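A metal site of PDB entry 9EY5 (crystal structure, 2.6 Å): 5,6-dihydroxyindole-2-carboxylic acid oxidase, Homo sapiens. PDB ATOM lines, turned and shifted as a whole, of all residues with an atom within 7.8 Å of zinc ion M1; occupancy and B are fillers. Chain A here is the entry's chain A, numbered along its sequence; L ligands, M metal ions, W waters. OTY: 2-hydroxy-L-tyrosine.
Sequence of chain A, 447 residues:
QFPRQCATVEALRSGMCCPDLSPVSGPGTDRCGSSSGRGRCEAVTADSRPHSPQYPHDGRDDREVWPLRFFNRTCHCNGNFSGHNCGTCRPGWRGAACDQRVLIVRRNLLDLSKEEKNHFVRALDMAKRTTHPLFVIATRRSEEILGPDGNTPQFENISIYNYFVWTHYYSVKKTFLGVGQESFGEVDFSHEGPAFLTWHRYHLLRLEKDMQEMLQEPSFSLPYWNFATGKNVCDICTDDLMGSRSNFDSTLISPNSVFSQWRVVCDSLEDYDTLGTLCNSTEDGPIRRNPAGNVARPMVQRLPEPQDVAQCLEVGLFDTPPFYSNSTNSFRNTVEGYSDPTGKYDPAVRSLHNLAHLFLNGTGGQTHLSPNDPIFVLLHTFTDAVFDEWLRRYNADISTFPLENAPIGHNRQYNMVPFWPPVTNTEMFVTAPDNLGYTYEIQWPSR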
ATOM      1  N   HIS A 168       7.620  28.964  16.973  1.00  0.00           N
ATOM      2  CA  HIS A 168       7.638  28.811  15.515  1.00  0.00           C
ATOM      3  C   HIS A 168       6.479  27.944  15.034  1.00  0.00           C
ATOM      4  O   HIS A 168       5.841  28.251  14.013  1.00  0.00           O
ATOM      5  CB  HIS A 168       8.983  28.239  15.106  1.00  0.00           C
ATOM      6  CG  HIS A 168       9.235  28.245  13.638  1.00  0.00           C
ATOM      7  ND1 HIS A 168       8.738  27.276  12.787  1.00  0.00           N
ATOM      8  CD2 HIS A 168      10.010  29.058  12.870  1.00  0.00           C
ATOM      9  CE1 HIS A 168       9.171  27.508  11.557  1.00  0.00           C
ATOM     10  NE2 HIS A 168       9.936  28.583  11.585  1.00  0.00           N
ATOM     11  N   SER A 171       3.190  29.879  15.145  1.00  0.00           N
ATOM     12  CA  SER A 171       3.035  30.883  14.098  1.00  0.00           C
ATOM     13  C   SER A 171       2.640  30.297  12.737  1.00  0.00           C
ATOM     14  O   SER A 171       2.141  31.058  11.896  1.00  0.00           O
ATOM     15  CB  SER A 171       4.320  31.700  13.959  1.00  0.00           C
ATOM     16  OG  SER A 171       5.383  30.895  13.482  1.00  0.00           O
ATOM     17  N   VAL A 172       2.831  28.994  12.491  1.00  0.00           N
ATOM     18  CA  VAL A 172       2.525  28.398  11.198  1.00  0.00           C
ATOM     19  C   VAL A 172       1.379  27.392  11.230  1.00  0.00           C
ATOM     20  O   VAL A 172       0.906  26.999  10.142  1.00  0.00           O
ATOM     21  CB  VAL A 172       3.755  27.733  10.546  1.00  0.00           C
ATOM     22  CG1 VAL A 172       4.949  28.659  10.533  1.00  0.00           C
ATOM     23  CG2 VAL A 172       4.075  26.360  11.218  1.00  0.00           C
ATOM     24  N   ASP A 188       0.069  31.767   7.407  1.00  0.00           N
ATOM     25  CA  ASP A 188       1.413  31.627   7.940  1.00  0.00           C
ATOM     26  C   ASP A 188       1.859  32.985   8.493  1.00  0.00           C
ATOM     27  O   ASP A 188       2.176  33.896   7.726  1.00  0.00           O
ATOM     28  CB  ASP A 188       2.352  31.115   6.863  1.00  0.00           C
ATOM     29  CG  ASP A 188       3.675  30.625   7.406  1.00  0.00           C
ATOM     30  OD1 ASP A 188       4.143  31.230   8.412  1.00  0.00           O
ATOM     31  OD2 ASP A 188       4.251  29.651   6.819  1.00  0.00           O
ATOM     32  N   SER A 190       4.564  33.866   9.889  1.00  0.00           N
ATOM     33  CA  SER A 190       5.991  34.139   9.935  1.00  0.00           C
ATOM     34  C   SER A 190       6.726  33.807   8.644  1.00  0.00           C
ATOM     35  O   SER A 190       7.957  33.933   8.618  1.00  0.00           O
ATOM     36  CB  SER A 190       6.634  33.378  11.091  1.00  0.00           C
ATOM     37  OG  SER A 190       6.144  32.044  11.156  1.00  0.00           O
ATOM     38  N   HIS A 191       6.028  33.390   7.586  1.00  0.00           N
ATOM     39  CA  HIS A 191       6.619  33.160   6.279  1.00  0.00           C
ATOM     40  C   HIS A 191       5.661  33.646   5.219  1.00  0.00           C
ATOM     41  O   HIS A 191       4.485  33.917   5.493  1.00  0.00           O
ATOM     42  CB  HIS A 191       6.927  31.689   6.035  1.00  0.00           C
ATOM     43  CG  HIS A 191       7.483  31.003   7.242  1.00  0.00           C
ATOM     44  ND1 HIS A 191       6.703  30.621   8.305  1.00  0.00           N
ATOM     45  CD2 HIS A 191       8.759  30.699   7.573  1.00  0.00           C
ATOM     46  CE1 HIS A 191       7.465  30.079   9.233  1.00  0.00           C
ATOM     47  NE2 HIS A 191       8.716  30.099   8.810  1.00  0.00           N
ATOM     48  N   PHE A 196       8.276  37.853   7.497  1.00  0.00           N
ATOM     49  CA  PHE A 196       9.188  36.719   7.605  1.00  0.00           C
ATOM     50  C   PHE A 196      10.534  37.112   8.209  1.00  0.00           C
ATOM     51  O   PHE A 196      11.011  36.471   9.157  1.00  0.00           O
ATOM     52  CB  PHE A 196       9.400  36.081   6.219  1.00  0.00           C
ATOM     53  CG  PHE A 196      10.644  35.233   6.127  1.00  0.00           C
ATOM     54  CD1 PHE A 196      10.668  33.950   6.682  1.00  0.00           C
ATOM     55  CD2 PHE A 196      11.787  35.708   5.497  1.00  0.00           C
ATOM     56  CE1 PHE A 196      11.816  33.171   6.595  1.00  0.00           C
ATOM     57  CE2 PHE A 196      12.936  34.921   5.405  1.00  0.00           C
ATOM     58  CZ  PHE A 196      12.950  33.657   5.966  1.00  0.00           C
ATOM     59  N   TRP A 199      10.114  38.635  11.944  1.00  0.00           N
ATOM     60  CA  TRP A 199       9.666  37.622  12.889  1.00  0.00           C
ATOM     61  C   TRP A 199      10.848  36.758  13.313  1.00  0.00           C
ATOM     62  O   TRP A 199      11.102  36.564  14.508  1.00  0.00           O
ATOM     63  CB  TRP A 199       8.550  36.779  12.275  1.00  0.00           C
ATOM     64  CG  TRP A 199       7.857  35.834  13.253  1.00  0.00           C
ATOM     65  CD1 TRP A 199       6.638  36.020  13.825  1.00  0.00           C
ATOM     66  CD2 TRP A 199       8.348  34.577  13.750  1.00  0.00           C
ATOM     67  NE1 TRP A 199       6.323  34.958  14.654  1.00  0.00           N
ATOM     68  CE2 TRP A 199       7.360  34.065  14.625  1.00  0.00           C
ATOM     69  CE3 TRP A 199       9.515  33.839  13.535  1.00  0.00           C
ATOM     70  CZ2 TRP A 199       7.521  32.846  15.290  1.00  0.00           C
ATOM     71  CZ3 TRP A 199       9.667  32.631  14.200  1.00  0.00           C
ATOM     72  CH2 TRP A 199       8.674  32.151  15.063  1.00  0.00           C
ATOM     73  N   HIS A 200      11.601  36.263  12.338  1.00  0.00           N
ATOM     74  CA  HIS A 200      12.736  35.405  12.636  1.00  0.00           C
ATOM     75  C   HIS A 200      13.873  36.166  13.304  1.00  0.00           C
ATOM     76  O   HIS A 200      14.587  35.593  14.141  1.00  0.00           O
ATOM     77  CB  HIS A 200      13.226  34.744  11.354  1.00  0.00           C
ATOM     78  CG  HIS A 200      12.335  33.656  10.874  1.00  0.00           C
ATOM     79  ND1 HIS A 200      11.265  33.875  10.026  1.00  0.00           N
ATOM     80  CD2 HIS A 200      12.365  32.321  11.112  1.00  0.00           C
ATOM     81  CE1 HIS A 200      10.676  32.722   9.772  1.00  0.00           C
ATOM     82  NE2 HIS A 200      11.319  31.767  10.424  1.00  0.00           N
ATOM     83  N   HIS A 203      12.839  36.173  16.830  1.00  0.00           N
ATOM     84  CA  HIS A 203      12.954  34.780  17.241  1.00  0.00           C
ATOM     85  C   HIS A 203      14.362  34.484  17.747  1.00  0.00           C
ATOM     86  O   HIS A 203      14.548  33.964  18.855  1.00  0.00           O
ATOM     87  CB  HIS A 203      12.594  33.890  16.049  1.00  0.00           C
ATOM     88  CG  HIS A 203      12.274  32.477  16.408  1.00  0.00           C
ATOM     89  ND1 HIS A 203      12.584  31.425  15.580  1.00  0.00           N
ATOM     90  CD2 HIS A 203      11.645  31.944  17.489  1.00  0.00           C
ATOM     91  CE1 HIS A 203      12.163  30.295  16.130  1.00  0.00           C
ATOM     92  NE2 HIS A 203      11.595  30.587  17.296  1.00  0.00           N
ATOM     93  N   GLU A 336      14.023  35.067   1.286  1.00  0.00           N
ATOM     94  CA  GLU A 336      13.251  33.938   1.786  1.00  0.00           C
ATOM     95  C   GLU A 336      13.396  32.728   0.857  1.00  0.00           C
ATOM     96  O   GLU A 336      13.517  31.593   1.318  1.00  0.00           O
ATOM     97  CB  GLU A 336      11.778  34.316   1.954  1.00  0.00           C
ATOM     98  CG  GLU A 336      10.951  33.208   2.628  1.00  0.00           C
ATOM     99  CD  GLU A 336       9.539  33.645   2.990  1.00  0.00           C
ATOM    100  OE1 GLU A 336       9.149  34.768   2.604  1.00  0.00           O
ATOM    101  OE2 GLU A 336       8.811  32.878   3.664  1.00  0.00           O
ATOM    102  N   HIS A 353      17.345  31.016   1.510  1.00  0.00           N
ATOM    103  CA  HIS A 353      16.866  30.478   2.790  1.00  0.00           C
ATOM    104  C   HIS A 353      16.013  29.233   2.584  1.00  0.00           C
ATOM    105  O   HIS A 353      16.163  28.249   3.330  1.00  0.00           O
ATOM    106  CB  HIS A 353      16.068  31.539   3.565  1.00  0.00           C
ATOM    107  CG  HIS A 353      14.965  30.981   4.433  1.00  0.00           C
ATOM    108  ND1 HIS A 353      13.731  30.622   3.923  1.00  0.00           N
ATOM    109  CD2 HIS A 353      14.904  30.719   5.758  1.00  0.00           C
ATOM    110  CE1 HIS A 353      12.966  30.170   4.895  1.00  0.00           C
ATOM    111  NE2 HIS A 353      13.645  30.231   6.010  1.00  0.00           N
ATOM    112  N   ASN A 354      15.105  29.245   1.606  1.00  0.00           N
ATOM    113  CA  ASN A 354      14.278  28.057   1.358  1.00  0.00           C
ATOM    114  C   ASN A 354      15.117  26.913   0.838  1.00  0.00           C
ATOM    115  O   ASN A 354      14.932  25.761   1.250  1.00  0.00           O
ATOM    116  CB  ASN A 354      13.155  28.359   0.359  1.00  0.00           C
ATOM    117  CG  ASN A 354      11.993  29.095   0.990  1.00  0.00           C
ATOM    118  OD1 ASN A 354      11.786  29.032   2.210  1.00  0.00           O
ATOM    119  ND2 ASN A 354      11.231  29.801   0.162  1.00  0.00           N
ATOM    120  N   HIS A 357      17.013  25.148   3.731  1.00  0.00           N
ATOM    121  CA  HIS A 357      16.177  24.213   4.470  1.00  0.00           C
ATOM    122  C   HIS A 357      16.015  22.880   3.736  1.00  0.00           C
ATOM    123  O   HIS A 357      16.209  21.812   4.310  1.00  0.00           O
ATOM    124  CB  HIS A 357      14.807  24.827   4.705  1.00  0.00           C
ATOM    125  CG  HIS A 357      14.721  25.690   5.908  1.00  0.00           C
ATOM    126  ND1 HIS A 357      14.362  25.201   7.154  1.00  0.00           N
ATOM    127  CD2 HIS A 357      14.889  27.014   6.063  1.00  0.00           C
ATOM    128  CE1 HIS A 357      14.341  26.192   8.017  1.00  0.00           C
ATOM    129  NE2 HIS A 357      14.669  27.303   7.389  1.00  0.00           N
ATOM    130  N   GLN A 366      10.730  20.490   7.330  1.00  0.00           N
ATOM    131  CA  GLN A 366       9.300  20.542   7.576  1.00  0.00           C
ATOM    132  C   GLN A 366       8.939  21.832   8.328  1.00  0.00           C
ATOM    133  O   GLN A 366       9.473  22.102   9.412  1.00  0.00           O
ATOM    134  CB  GLN A 366       8.903  19.298   8.353  1.00  0.00           C
ATOM    135  CG  GLN A 366       9.773  18.107   7.926  1.00  0.00           C
ATOM    136  CD  GLN A 366       9.294  16.787   8.477  1.00  0.00           C
ATOM    137  OE1 GLN A 366      10.020  16.123   9.235  1.00  0.00           O
ATOM    138  NE2 GLN A 366       8.075  16.405   8.112  1.00  0.00           N
ATOM    139  N   THR A 367       8.020  22.633   7.762  1.00  0.00           N
ATOM    140  CA  THR A 367       7.842  23.994   8.265  1.00  0.00           C
ATOM    141  C   THR A 367       7.373  24.005   9.720  1.00  0.00           C
ATOM    142  O   THR A 367       7.770  24.903  10.478  1.00  0.00           O
ATOM    143  CB  THR A 367       6.866  24.782   7.383  1.00  0.00           C
ATOM    144  OG1 THR A 367       7.330  24.776   6.026  1.00  0.00           O
ATOM    145  CG2 THR A 367       6.734  26.270   7.905  1.00  0.00           C
ATOM    146  N   SER A 370      10.899  22.521  11.770  1.00  0.00           N
ATOM    147  CA  SER A 370      12.295  22.784  11.412  1.00  0.00           C
ATOM    148  C   SER A 370      13.192  23.269  12.550  1.00  0.00           C
ATOM    149  O   SER A 370      14.345  22.821  12.605  1.00  0.00           O
ATOM    150  CB  SER A 370      12.347  23.770  10.234  1.00  0.00           C
ATOM    151  OG  SER A 370      11.401  24.799  10.418  1.00  0.00           O
ATOM    152  N   PRO A 371      12.760  24.144  13.472  1.00  0.00           N
ATOM    153  CA  PRO A 371      13.687  24.562  14.554  1.00  0.00           C
ATOM    154  C   PRO A 371      14.179  23.418  15.441  1.00  0.00           C
ATOM    155  O   PRO A 371      15.103  23.651  16.239  1.00  0.00           O
ATOM    156  CB  PRO A 371      12.861  25.575  15.360  1.00  0.00           C
ATOM    157  CG  PRO A 371      11.755  25.981  14.479  1.00  0.00           C
ATOM    158  CD  PRO A 371      11.462  24.832  13.594  1.00  0.00           C
ATOM    159  N   PHE A 376      18.891  25.080  12.366  1.00  0.00           N
ATOM    160  CA  PHE A 376      17.921  26.159  12.186  1.00  0.00           C
ATOM    161  C   PHE A 376      18.486  27.476  12.697  1.00  0.00           C
ATOM    162  O   PHE A 376      18.453  28.498  12.005  1.00  0.00           O
ATOM    163  CB  PHE A 376      16.617  25.828  12.913  1.00  0.00           C
ATOM    164  CG  PHE A 376      15.519  26.842  12.697  1.00  0.00           C
ATOM    165  CD1 PHE A 376      15.542  28.074  13.339  1.00  0.00           C
ATOM    166  CD2 PHE A 376      14.463  26.567  11.828  1.00  0.00           C
ATOM    167  CE1 PHE A 376      14.539  29.028  13.122  1.00  0.00           C
ATOM    168  CE2 PHE A 376      13.447  27.510  11.607  1.00  0.00           C
ATOM    169  CZ  PHE A 376      13.486  28.737  12.259  1.00  0.00           C
ATOM    170  N   HIS A 380      19.430  30.743  10.308  1.00  0.00           N
ATOM    171  CA  HIS A 380      18.686  31.986  10.412  1.00  0.00           C
ATOM    172  C   HIS A 380      19.514  33.158  10.863  1.00  0.00           C
ATOM    173  O   HIS A 380      19.237  34.288  10.434  1.00  0.00           O
ATOM    174  CB  HIS A 380      17.486  31.811  11.323  1.00  0.00           C
ATOM    175  CG  HIS A 380      16.334  31.281  10.562  1.00  0.00           C
ATOM    176  ND1 HIS A 380      15.528  32.097   9.779  1.00  0.00           N
ATOM    177  CD2 HIS A 380      15.954  30.014  10.300  1.00  0.00           C
ATOM    178  CE1 HIS A 380      14.655  31.347   9.144  1.00  0.00           C
ATOM    179  NE2 HIS A 380      14.897  30.090   9.450  1.00  0.00           N
HETATM  180  OD1 OTY L   1      11.283  23.684   4.114  1.00  0.00           O
HETATM  181  N   OTY L   1       9.560  25.759   0.348  1.00  0.00           N
HETATM  182  CA  OTY L   1       9.812  25.276   1.719  1.00  0.00           C
HETATM  183  C   OTY L   1       8.522  25.355   2.562  1.00  0.00           C
HETATM  184  O   OTY L   1       8.199  24.384   3.307  1.00  0.00           O
HETATM  185  CB  OTY L   1      10.984  26.092   2.402  1.00  0.00           C
HETATM  186  CG  OTY L   1      10.914  26.132   3.963  1.00  0.00           C
HETATM  187  CD1 OTY L   1      11.061  24.975   4.731  1.00  0.00           C
HETATM  188  CD2 OTY L   1      10.716  27.370   4.661  1.00  0.00           C
HETATM  189  CE1 OTY L   1      11.002  25.014   6.170  1.00  0.00           C
HETATM  190  CE2 OTY L   1      10.631  27.442   6.082  1.00  0.00           C
HETATM  191  CZ  OTY L   1      10.783  26.244   6.823  1.00  0.00           C
HETATM  192  OH  OTY L   1      10.723  26.245   8.280  1.00  0.00           O
HETATM  193  OXT OTY L   1       7.769  26.391   2.522  1.00  0.00           O
HETATM  194 ZN    ZN M   1      10.665  29.775   9.853  1.00  0.00          ZN
HETATM  195 ZN    ZN M   2      13.573  29.182   7.941  1.00  0.00          ZN
HETATM  196  O   HOH W   1      11.982  28.679   8.761  1.00  0.00           O
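The side-chain hydroxyl (OG1) of Thr 367 lies within hydrogen-bond range of an oxygen (O) of the ligand. The side-chain hydroxyl of Ser 370 lies within hydrogen-bond range of an oxygen (OH) of the ligand (2.7 Å).
ND1 of His 168 lies close to O of Thr 367 (3.4 Å). A ring nitrogen (ND1) of His 200 sits at hydrogen-bond distance from the backbone carbonyl oxygen (O) of Phe 196 (2.7 Å). OG of Ser 171 is in hydrogen-bond range of O of His 168 (2.7 Å). The side-chain hydroxyl (OG) of Ser 190 lies close to a ring nitrogen (ND1) of His 191. ND1 of His 191 is in hydrogen-bond range of OD1 of Asp 188 (2.6 Å).
Residues that only touch zinc ion M1: Phe 376 (3.9 Å).
Water W1 binds zinc ion M1, 2.0 Å away. NE2 of His 200 binds zinc ion M1 (2.2 Å). A ring nitrogen (NE2) of His 168 is bound to zinc ion M1. Zinc ion M1 is bound by NE2 of His 191, at 2.2 Å.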
